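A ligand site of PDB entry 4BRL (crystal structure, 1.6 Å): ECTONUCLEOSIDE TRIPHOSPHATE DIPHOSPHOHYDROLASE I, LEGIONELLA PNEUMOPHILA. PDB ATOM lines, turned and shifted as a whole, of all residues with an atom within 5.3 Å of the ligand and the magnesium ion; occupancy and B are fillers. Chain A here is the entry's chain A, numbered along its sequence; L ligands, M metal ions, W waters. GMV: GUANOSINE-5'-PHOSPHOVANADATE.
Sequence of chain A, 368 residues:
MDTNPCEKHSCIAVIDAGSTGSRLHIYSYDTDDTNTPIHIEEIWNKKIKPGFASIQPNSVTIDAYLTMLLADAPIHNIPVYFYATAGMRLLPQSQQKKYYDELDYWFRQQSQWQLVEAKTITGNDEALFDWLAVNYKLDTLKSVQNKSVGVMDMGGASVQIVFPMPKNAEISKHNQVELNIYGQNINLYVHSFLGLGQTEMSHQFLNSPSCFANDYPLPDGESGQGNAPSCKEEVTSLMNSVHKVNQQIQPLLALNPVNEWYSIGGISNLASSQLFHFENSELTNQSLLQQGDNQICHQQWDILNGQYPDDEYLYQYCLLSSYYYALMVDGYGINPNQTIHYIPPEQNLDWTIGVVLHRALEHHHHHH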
ATOM      1  N   ASP A  16      12.378  11.143   6.916  1.00  0.00           N
ATOM      2  CA  ASP A  16      11.276  10.827   5.931  1.00  0.00           C
ATOM      3  C   ASP A  16      11.253   9.321   5.842  1.00  0.00           C
ATOM      4  O   ASP A  16      12.119   8.734   5.142  1.00  0.00           O
ATOM      5  CB  ASP A  16      11.626  11.481   4.565  1.00  0.00           C
ATOM      6  CG  ASP A  16      10.776  11.024   3.381  1.00  0.00           C
ATOM      7  OD1 ASP A  16       9.804  10.275   3.539  1.00  0.00           O
ATOM      8  OD2 ASP A  16      11.101  11.415   2.224  1.00  0.00           O
ATOM      9  N   ALA A  17      10.238   8.704   6.440  1.00  0.00           N
ATOM     10  CA  ALA A  17      10.140   7.254   6.364  1.00  0.00           C
ATOM     11  C   ALA A  17       9.125   6.919   5.270  1.00  0.00           C
ATOM     12  O   ALA A  17       7.894   6.731   5.548  1.00  0.00           O
ATOM     13  CB  ALA A  17       9.739   6.658   7.722  1.00  0.00           C
ATOM     14  N   GLY A  18       9.638   6.910   4.045  1.00  0.00           N
ATOM     15  CA  GLY A  18       8.796   6.728   2.838  1.00  0.00           C
ATOM     16  C   GLY A  18       8.530   5.281   2.478  1.00  0.00           C
ATOM     17  O   GLY A  18       9.133   4.341   3.060  1.00  0.00           O
ATOM     18  N   SER A  19       7.717   5.093   1.433  1.00  0.00           N
ATOM     19  CA  SER A  19       7.314   3.719   1.096  1.00  0.00           C
ATOM     20  C   SER A  19       8.481   2.888   0.570  1.00  0.00           C
ATOM     21  O   SER A  19       8.497   1.627   0.739  1.00  0.00           O
ATOM     22  CB  SER A  19       6.155   3.742   0.080  1.00  0.00           C
ATOM     23  OG  SER A  19       6.571   4.219  -1.147  1.00  0.00           O
ATOM     24  N   THR A  20       9.472   3.541  -0.060  1.00  0.00           N
ATOM     25  CA  THR A  20      10.540   2.781  -0.735  1.00  0.00           C
ATOM     26  C   THR A  20      11.857   2.875   0.029  1.00  0.00           C
ATOM     27  O   THR A  20      12.833   2.203  -0.317  1.00  0.00           O
ATOM     28  CB  THR A  20      10.761   3.249  -2.196  1.00  0.00           C
ATOM     29  OG1 THR A  20      11.201   4.605  -2.202  1.00  0.00           O
ATOM     30  CG2 THR A  20       9.525   3.103  -3.037  1.00  0.00           C
ATOM     31  N   GLY A  21      11.884   3.689   1.095  1.00  0.00           N
ATOM     32  CA  GLY A  21      13.136   3.847   1.851  1.00  0.00           C
ATOM     33  C   GLY A  21      13.013   4.964   2.912  1.00  0.00           C
ATOM     34  O   GLY A  21      12.014   5.689   2.923  1.00  0.00           O
ATOM     35  N   ARG A  23      14.993   8.372   4.776  1.00  0.00           N
ATOM     36  CA  ARG A  23      16.050   9.366   4.534  1.00  0.00           C
ATOM     37  C   ARG A  23      16.157  10.212   5.823  1.00  0.00           C
ATOM     38  O   ARG A  23      15.189  10.899   6.199  1.00  0.00           O
ATOM     39  CB  ARG A  23      15.754  10.258   3.336  1.00  0.00           C
ATOM     40  CG  ARG A  23      15.455   9.466   2.067  1.00  0.00           C
ATOM     41  CD  ARG A  23      13.929   9.252   1.960  1.00  0.00           C
ATOM     42  NE  ARG A  23      13.648   8.253   0.919  1.00  0.00           N
ATOM     43  CZ  ARG A  23      12.441   7.955   0.491  1.00  0.00           C
ATOM     44  NH1 ARG A  23      11.369   8.661   0.947  1.00  0.00           N
ATOM     45  NH2 ARG A  23      12.344   6.969  -0.407  1.00  0.00           N
ATOM     46  N   THR A  85       5.266   8.126   5.950  1.00  0.00           N
ATOM     47  CA  THR A  85       4.263   8.537   4.978  1.00  0.00           C
ATOM     48  C   THR A  85       3.438   7.369   4.414  1.00  0.00           C
ATOM     49  O   THR A  85       2.952   6.543   5.224  1.00  0.00           O
ATOM     50  CB  THR A  85       4.854   9.450   3.906  1.00  0.00           C
ATOM     51  OG1 THR A  85       5.933   8.783   3.240  1.00  0.00           O
ATOM     52  CG2 THR A  85       5.396  10.776   4.530  1.00  0.00           C
ATOM     53  N   ALA A  86       3.271   7.262   3.090  1.00  0.00           N
ATOM     54  CA  ALA A  86       2.148   6.390   2.598  1.00  0.00           C
ATOM     55  C   ALA A  86       2.416   4.881   2.749  1.00  0.00           C
ATOM     56  O   ALA A  86       1.450   4.103   2.827  1.00  0.00           O
ATOM     57  CB  ALA A  86       1.840   6.704   1.131  1.00  0.00           C
ATOM     58  N   GLY A  87       3.685   4.463   2.852  1.00  0.00           N
ATOM     59  CA  GLY A  87       3.965   3.042   3.069  1.00  0.00           C
ATOM     60  C   GLY A  87       3.273   2.594   4.399  1.00  0.00           C
ATOM     61  O   GLY A  87       2.597   1.517   4.468  1.00  0.00           O
ATOM     62  N   ARG A  89       0.778   4.270   5.851  1.00  0.00           N
ATOM     63  CA  ARG A  89      -0.683   4.493   5.708  1.00  0.00           C
ATOM     64  C   ARG A  89      -1.413   3.285   5.089  1.00  0.00           C
ATOM     65  O   ARG A  89      -2.644   3.203   5.186  1.00  0.00           O
ATOM     66  CB  ARG A  89      -0.997   5.734   4.877  1.00  0.00           C
ATOM     67  CG  ARG A  89      -0.550   7.027   5.619  1.00  0.00           C
ATOM     68  CD  ARG A  89      -1.076   8.395   5.164  1.00  0.00           C
ATOM     69  NE  ARG A  89      -0.598   8.794   3.879  1.00  0.00           N
ATOM     70  CZ  ARG A  89       0.459   9.579   3.525  1.00  0.00           C
ATOM     71  NH1 ARG A  89       1.306  10.209   4.300  1.00  0.00           N
ATOM     72  NH2 ARG A  89       0.620   9.691   2.256  1.00  0.00           N
ATOM     73  N   GLU A 126       1.598  15.737   4.493  1.00  0.00           N
ATOM     74  CA  GLU A 126       2.737  15.496   3.598  1.00  0.00           C
ATOM     75  C   GLU A 126       2.705  16.538   2.435  1.00  0.00           C
ATOM     76  O   GLU A 126       3.749  17.110   2.053  1.00  0.00           O
ATOM     77  CB  GLU A 126       2.666  14.090   3.029  1.00  0.00           C
ATOM     78  CG  GLU A 126       3.893  13.622   2.240  1.00  0.00           C
ATOM     79  CD  GLU A 126       3.728  12.148   1.799  1.00  0.00           C
ATOM     80  OE1 GLU A 126       2.705  11.554   2.194  1.00  0.00           O
ATOM     81  OE2 GLU A 126       4.586  11.596   1.110  1.00  0.00           O
ATOM     82  N   ASP A 153       4.282  15.843  -5.695  1.00  0.00           N
ATOM     83  CA  ASP A 153       5.259  14.907  -5.129  1.00  0.00           C
ATOM     84  C   ASP A 153       4.823  13.503  -5.569  1.00  0.00           C
ATOM     85  O   ASP A 153       3.702  13.061  -5.252  1.00  0.00           O
ATOM     86  CB  ASP A 153       5.324  15.075  -3.600  1.00  0.00           C
ATOM     87  CG  ASP A 153       6.239  14.057  -2.914  1.00  0.00           C
ATOM     88  OD1 ASP A 153       6.511  12.956  -3.469  1.00  0.00           O
ATOM     89  OD2 ASP A 153       6.613  14.293  -1.749  1.00  0.00           O
ATOM     90  N   MET A 154       5.697  12.878  -6.372  1.00  0.00           N
ATOM     91  CA  MET A 154       5.463  11.559  -6.946  1.00  0.00           C
ATOM     92  C   MET A 154       6.149  10.497  -6.079  1.00  0.00           C
ATOM     93  O   MET A 154       7.366  10.277  -6.176  1.00  0.00           O
ATOM     94  CB  MET A 154       6.067  11.515  -8.367  1.00  0.00           C
ATOM     95  CG  MET A 154       5.664  12.615  -9.381  1.00  0.00           C
ATOM     96  SD  MET A 154       3.916  12.765  -9.452  1.00  0.00           S
ATOM     97  CE  MET A 154       3.690  13.982 -10.810  1.00  0.00           C
ATOM     98  N   GLY A 155       5.344   9.807  -5.261  1.00  0.00           N
ATOM     99  CA  GLY A 155       5.922   8.847  -4.355  1.00  0.00           C
ATOM    100  C   GLY A 155       5.684   7.384  -4.794  1.00  0.00           C
ATOM    101  O   GLY A 155       5.040   7.137  -5.810  1.00  0.00           O
ATOM    102  N   GLY A 156       6.125   6.438  -3.957  1.00  0.00           N
ATOM    103  CA  GLY A 156       5.920   5.017  -4.286  1.00  0.00           C
ATOM    104  C   GLY A 156       4.515   4.463  -3.964  1.00  0.00           C
ATOM    105  O   GLY A 156       4.099   3.499  -4.603  1.00  0.00           O
ATOM    106  N   ALA A 157       3.806   5.072  -2.986  1.00  0.00           N
ATOM    107  CA  ALA A 157       2.458   4.616  -2.577  1.00  0.00           C
ATOM    108  C   ALA A 157       1.406   5.701  -2.723  1.00  0.00           C
ATOM    109  O   ALA A 157       0.231   5.372  -2.977  1.00  0.00           O
ATOM    110  CB  ALA A 157       2.445   4.013  -1.165  1.00  0.00           C
ATOM    111  N   SER A 158       1.792   6.985  -2.522  1.00  0.00           N
ATOM    112  CA  SER A 158       0.858   8.069  -2.768  1.00  0.00           C
ATOM    113  C   SER A 158       1.490   9.155  -3.653  1.00  0.00           C
ATOM    114  O   SER A 158       2.690   9.193  -3.832  1.00  0.00           O
ATOM    115  CB  SER A 158       0.427   8.738  -1.430  1.00  0.00           C
ATOM    116  OG  SER A 158       1.571   9.428  -0.864  1.00  0.00           O
ATOM    117  N   GLN A 160       1.055  13.535  -4.136  1.00  0.00           N
ATOM    118  CA  GLN A 160       0.383  14.770  -3.630  1.00  0.00           C
ATOM    119  C   GLN A 160       0.360  15.822  -4.708  1.00  0.00           C
ATOM    120  O   GLN A 160       1.303  15.899  -5.557  1.00  0.00           O
ATOM    121  CB  GLN A 160       1.101  15.394  -2.394  1.00  0.00           C
ATOM    122  CG  GLN A 160       0.975  14.553  -1.075  1.00  0.00           C
ATOM    123  CD  GLN A 160       1.780  13.203  -1.131  1.00  0.00           C
ATOM    124  OE1 GLN A 160       1.164  12.101  -1.207  1.00  0.00           O
ATOM    125  NE2 GLN A 160       3.148  13.275  -1.201  1.00  0.00           N
ATOM    126  N   GLN A 198       3.863   5.040  -7.458  1.00  0.00           N
ATOM    127  CA  GLN A 198       4.388   4.224  -8.519  1.00  0.00           C
ATOM    128  C   GLN A 198       4.353   2.720  -8.224  1.00  0.00           C
ATOM    129  O   GLN A 198       3.988   1.912  -9.111  1.00  0.00           O
ATOM    130  CB  GLN A 198       5.765   4.749  -8.978  1.00  0.00           C
ATOM    131  CG  GLN A 198       6.951   3.910  -8.695  1.00  0.00           C
ATOM    132  CD  GLN A 198       8.247   4.410  -9.313  1.00  0.00           C
ATOM    133  OE1 GLN A 198       8.481   5.646  -9.379  1.00  0.00           O
ATOM    134  NE2 GLN A 198       9.098   3.474  -9.755  1.00  0.00           N
ATOM    135  N   THR A 199       4.705   2.321  -7.007  1.00  0.00           N
ATOM    136  CA  THR A 199       4.721   0.860  -6.722  1.00  0.00           C
ATOM    137  C   THR A 199       3.305   0.298  -6.721  1.00  0.00           C
ATOM    138  O   THR A 199       3.067  -0.772  -7.335  1.00  0.00           O
ATOM    139  CB  THR A 199       5.327   0.590  -5.309  1.00  0.00           C
ATOM    140  OG1 THR A 199       6.600   1.226  -5.267  1.00  0.00           O
ATOM    141  CG2 THR A 199       5.451  -0.912  -4.986  1.00  0.00           C
ATOM    142  N   GLY A 265      10.220  13.854  -6.026  1.00  0.00           N
ATOM    143  CA  GLY A 265       9.897  12.407  -5.973  1.00  0.00           C
ATOM    144  C   GLY A 265      10.489  11.718  -7.179  1.00  0.00           C
ATOM    145  O   GLY A 265      11.466  12.220  -7.788  1.00  0.00           O
ATOM    146  N   GLY A 266       9.849  10.613  -7.575  1.00  0.00           N
ATOM    147  CA  GLY A 266      10.444   9.667  -8.535  1.00  0.00           C
ATOM    148  C   GLY A 266      10.651  10.238  -9.959  1.00  0.00           C
ATOM    149  O   GLY A 266      11.519   9.766 -10.718  1.00  0.00           O
ATOM    150  N   ASN A 269      14.114  11.407 -10.691  1.00  0.00           N
ATOM    151  CA  ASN A 269      15.020  10.324 -11.013  1.00  0.00           C
ATOM    152  C   ASN A 269      14.863   9.824 -12.439  1.00  0.00           C
ATOM    153  O   ASN A 269      15.884   9.629 -13.137  1.00  0.00           O
ATOM    154  CB  ASN A 269      14.905   9.196  -9.992  1.00  0.00           C
ATOM    155  CG  ASN A 269      15.008   9.698  -8.558  1.00  0.00           C
ATOM    156  OD1 ASN A 269      13.998  10.027  -7.933  1.00  0.00           O
ATOM    157  ND2 ASN A 269      16.253   9.759  -8.025  1.00  0.00           N
ATOM    158  N   LEU A 270      13.635   9.637 -12.892  1.00  0.00           N
ATOM    159  CA  LEU A 270      13.403   9.225 -14.288  1.00  0.00           C
ATOM    160  C   LEU A 270      13.928  10.258 -15.263  1.00  0.00           C
ATOM    161  O   LEU A 270      14.677   9.937 -16.214  1.00  0.00           O
ATOM    162  CB  LEU A 270      11.882   8.993 -14.588  1.00  0.00           C
ATOM    163  CG  LEU A 270      11.425   8.428 -15.956  1.00  0.00           C
ATOM    164  CD1 LEU A 270      11.885   7.009 -16.059  1.00  0.00           C
ATOM    165  CD2 LEU A 270       9.911   8.441 -16.190  1.00  0.00           C
ATOM    166  N   TYR A 313      15.490   0.466 -11.678  1.00  0.00           N
ATOM    167  CA  TYR A 313      14.089   0.725 -12.038  1.00  0.00           C
ATOM    168  C   TYR A 313      13.818   0.748 -13.520  1.00  0.00           C
ATOM    169  O   TYR A 313      12.646   0.958 -13.992  1.00  0.00           O
ATOM    170  CB  TYR A 313      13.581   2.024 -11.491  1.00  0.00           C
ATOM    171  CG  TYR A 313      12.953   1.921 -10.142  1.00  0.00           C
ATOM    172  CD1 TYR A 313      11.808   1.147  -9.935  1.00  0.00           C
ATOM    173  CD2 TYR A 313      13.462   2.634  -9.073  1.00  0.00           C
ATOM    174  CE1 TYR A 313      11.226   1.053  -8.684  1.00  0.00           C
ATOM    175  CE2 TYR A 313      12.885   2.549  -7.821  1.00  0.00           C
ATOM    176  CZ  TYR A 313      11.770   1.774  -7.629  1.00  0.00           C
ATOM    177  OH  TYR A 313      11.207   1.770  -6.363  1.00  0.00           O
ATOM    178  N   TYR A 317      10.483   1.804 -16.828  1.00  0.00           N
ATOM    179  CA  TYR A 317      10.553   3.146 -17.437  1.00  0.00           C
ATOM    180  C   TYR A 317       9.463   3.400 -18.545  1.00  0.00           C
ATOM    181  O   TYR A 317       8.955   4.499 -18.685  1.00  0.00           O
ATOM    182  CB  TYR A 317      11.953   3.427 -18.005  1.00  0.00           C
ATOM    183  CG  TYR A 317      12.999   3.818 -16.956  1.00  0.00           C
ATOM    184  CD1 TYR A 317      12.733   3.751 -15.547  1.00  0.00           C
ATOM    185  CD2 TYR A 317      14.234   4.248 -17.360  1.00  0.00           C
ATOM    186  CE1 TYR A 317      13.713   4.096 -14.623  1.00  0.00           C
ATOM    187  CE2 TYR A 317      15.216   4.582 -16.457  1.00  0.00           C
ATOM    188  CZ  TYR A 317      14.955   4.530 -15.104  1.00  0.00           C
ATOM    189  OH  TYR A 317      15.958   4.881 -14.243  1.00  0.00           O
ATOM    190  N   TRP A 351      10.116  16.675   1.551  1.00  0.00           N
ATOM    191  CA  TRP A 351       9.225  17.561   2.259  1.00  0.00           C
ATOM    192  C   TRP A 351       9.778  17.890   3.673  1.00  0.00           C
ATOM    193  O   TRP A 351       9.111  18.633   4.430  1.00  0.00           O
ATOM    194  CB  TRP A 351       7.826  16.924   2.366  1.00  0.00           C
ATOM    195  CG  TRP A 351       7.871  15.460   2.785  1.00  0.00           C
ATOM    196  CD1 TRP A 351       7.841  14.360   1.940  1.00  0.00           C
ATOM    197  CD2 TRP A 351       8.032  14.937   4.133  1.00  0.00           C
ATOM    198  NE1 TRP A 351       7.905  13.211   2.674  1.00  0.00           N
ATOM    199  CE2 TRP A 351       8.021  13.497   3.994  1.00  0.00           C
ATOM    200  CE3 TRP A 351       8.066  15.505   5.432  1.00  0.00           C
ATOM    201  CZ2 TRP A 351       8.131  12.634   5.089  1.00  0.00           C
ATOM    202  CZ3 TRP A 351       8.204  14.653   6.521  1.00  0.00           C
ATOM    203  CH2 TRP A 351       8.221  13.225   6.347  1.00  0.00           C
HETATM  204  VB  GMV L   1       5.575   7.918  -0.344  1.00  0.00           V
HETATM  205  O1B GMV L   1       4.403   7.192  -1.319  1.00  0.00           O
HETATM  206  O2B GMV L   1       5.827   7.148   1.186  1.00  0.00           O
HETATM  207  O3B GMV L   1       6.305   9.583  -0.818  1.00  0.00           O
HETATM  208  O4B GMV L   1       4.003   9.132   0.568  1.00  0.00           O
HETATM  209  PA  GMV L   1       8.676   7.372  -1.383  1.00  0.00           P
HETATM  210  O1A GMV L   1       9.561   6.249  -0.963  1.00  0.00           O
HETATM  211  O2A GMV L   1       9.027   8.682  -0.704  1.00  0.00           O
HETATM  212  O3A GMV L   1       7.175   6.990  -1.130  1.00  0.00           O
HETATM  213  O5' GMV L   1       8.767   7.568  -2.956  1.00  0.00           O
HETATM  214  C5' GMV L   1       9.965   8.000  -3.665  1.00  0.00           C
HETATM  215  C4' GMV L   1       9.721   7.652  -5.104  1.00  0.00           C
HETATM  216  O4' GMV L   1      10.933   7.947  -5.827  1.00  0.00           O
HETATM  217  C3' GMV L   1       9.461   6.133  -5.300  1.00  0.00           C
HETATM  218  O3' GMV L   1       8.460   5.905  -6.306  1.00  0.00           O
HETATM  219  C2' GMV L   1      10.796   5.596  -5.784  1.00  0.00           C
HETATM  220  O2' GMV L   1      10.688   4.407  -6.588  1.00  0.00           O
HETATM  221  C1' GMV L   1      11.399   6.791  -6.509  1.00  0.00           C
HETATM  222  N9  GMV L   1      12.840   6.676  -6.363  1.00  0.00           N
HETATM  223  C8  GMV L   1      13.609   6.723  -5.232  1.00  0.00           C
HETATM  224  N7  GMV L   1      14.916   6.537  -5.561  1.00  0.00           N
HETATM  225  C5  GMV L   1      15.010   6.360  -6.935  1.00  0.00           C
HETATM  226  C6  GMV L   1      16.099   6.109  -7.952  1.00  0.00           C
HETATM  227  O6  GMV L   1      17.295   6.028  -7.552  1.00  0.00           O
HETATM  228  N1  GMV L   1      15.785   5.971  -9.285  1.00  0.00           N
HETATM  229  C2  GMV L   1      14.476   6.059  -9.676  1.00  0.00           C
HETATM  230  N2  GMV L   1      14.179   5.954 -10.964  1.00  0.00           N
HETATM  231  N3  GMV L   1      13.416   6.321  -8.801  1.00  0.00           N
HETATM  232  C4  GMV L   1      13.630   6.460  -7.460  1.00  0.00           C
HETATM  233 MG    MG M   1       8.092  10.492  -0.439  1.00  0.00          MG
HETATM  234  O   HOH W   1       8.300  11.157  -2.408  1.00  0.00           O
HETATM  235  O   HOH W   2      10.858   7.012 -11.103  1.00  0.00           O
HETATM  236  O   HOH W   3       9.848  11.524   0.065  1.00  0.00           O
HETATM  237  O   HOH W   4       4.451  11.035  -2.332  1.00  0.00           O
HETATM  238  O   HOH W   5       7.906  10.161   1.732  1.00  0.00           O
HETATM  239  O   HOH W   6       6.866  12.180  -0.050  1.00  0.00           O
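N of Gly 266 lies close to O4' of the ligand (3.4 Å). The side-chain hydroxyl (OG1) of Thr 20 is in hydrogen-bond range of an oxygen (O1A) of the ligand, at 2.6 Å. O1A of the ligand lies within hydrogen-bond range of N of Ser 19, at 3.2 Å. The side-chain hydroxyl of Thr 85 sits close to an oxygen (O2B) of the ligand, 2.6 Å away. The backbone NH (N) of Gly 156 lies within hydrogen-bond range of an oxygen (O5') of the ligand. O3' of the ligand lies within hydrogen-bond range of OE1 of Gln 198. The side-chain hydroxyl (OH) of Tyr 313 sits at hydrogen-bond distance from an oxygen (O2') of the ligand (2.7 Å). OE2 of Glu 126 sits close to O4B of the ligand, 2.6 Å away. O1A of the ligand is in hydrogen-bond range of N of Thr 20 (2.9 Å). NH2 of Arg 23 is in salt-bridge range of O1A of the ligand (2.9 Å).
The side-chain hydroxyl (OG1) of Thr 20 sits at hydrogen-bond distance from the guanidinium group (NH2) of Arg 23, 3.2 Å away. The guanidinium group (NH2) of Arg 89 sits at hydrogen-bond distance from the side-chain hydroxyl (OG) of Ser 158 (3.3 Å). O of Gly 265 sits close to OD1 of Asn 269. The backbone NH (N) of Thr 199 is in hydrogen-bond range of the backbone carbonyl oxygen (O) of Gly 156 (2.7 Å). N of Gln 198 is in hydrogen-bond range of O of Gly 155 (2.9 Å). OG of Ser 158 is in hydrogen-bond range of OE1 of Gln 160 (2.7 Å). OE1 of Glu 126 is in salt-bridge range of NH2 of Arg 89, at 2.8 Å. The backbone carbonyl oxygen of Gly 156 lies within hydrogen-bond range of the backbone NH of Gln 198 (3.3 Å).
An oxygen (O2B) of the ligand sits close to the backbone NH (N) of Ala 86. An oxygen (O1B) of the ligand sits close to the backbone NH (N) of Ala 157, at 2.8 Å. The side-chain hydroxyl (OG) of Ser 158 sits close to an oxygen (O4B) of the ligand, 2.8 Å away. Residues that only touch the ligand: Gly 18 (3.4 Å), Gly 87 (3.8 Å), Arg 89 (3.8 Å), Met 154 (3.7 Å), Gly 155 (3.4 Å), Asn 269 (3.2 Å) and Tyr 317 (3.9 Å). Hydrophobic or aromatic side chains within 4 Å of the ligand: Ala 86, Ala 157 and Tyr 313. Within 4 Å of the ligand: Gly 18, Ser 19, Thr 20, Arg 23, Thr 85, Ala 86, Gly 87, Arg 89, Glu 126, Met 154, Gly 155, Gly 156, Ala 157, Ser 158, Gln 198, Gly 266, Asn 269, Tyr 313 and Tyr 317. The nearest printed residue that does not touch the ligand is Gly 21 (4.02 Å).
Merely in contact with the magnesium ion: Glu 126.
The magnesium ion is bound by an oxygen (O3B) of the ligand (2.0 Å), an oxygen (O2A) of the ligand (2.1 Å), water W1 (2.1 Å), water W3 (2.1 Å), water W6 (2.1 Å) and water W5 (2.2 Å).
Water W6 lies within hydrogen-bond range of the side-chain carboxylate of Glu 126, the side-chain carboxylate of Asp 153 and the indole nitrogen of Trp 351. Water W3 lies within hydrogen-bond range of OD2 of Asp 16 (2.5 Å) and NH1 of Arg 23 (3.4 Å). Water W5 lies within hydrogen-bond range of OD1 of Asp 16 (2.6 Å), OG1 of Thr 85 (2.8 Å) and NE1 of Trp 351 (3.2 Å). Water W2 lies within hydrogen-bond range of the backbone carbonyl oxygen (O) of Gly 266 (2.9 Å), the side-chain amide oxygen (OE1) of Gln 198 (3.2 Å) and a nitrogen (N2) of the ligand (3.5 Å).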
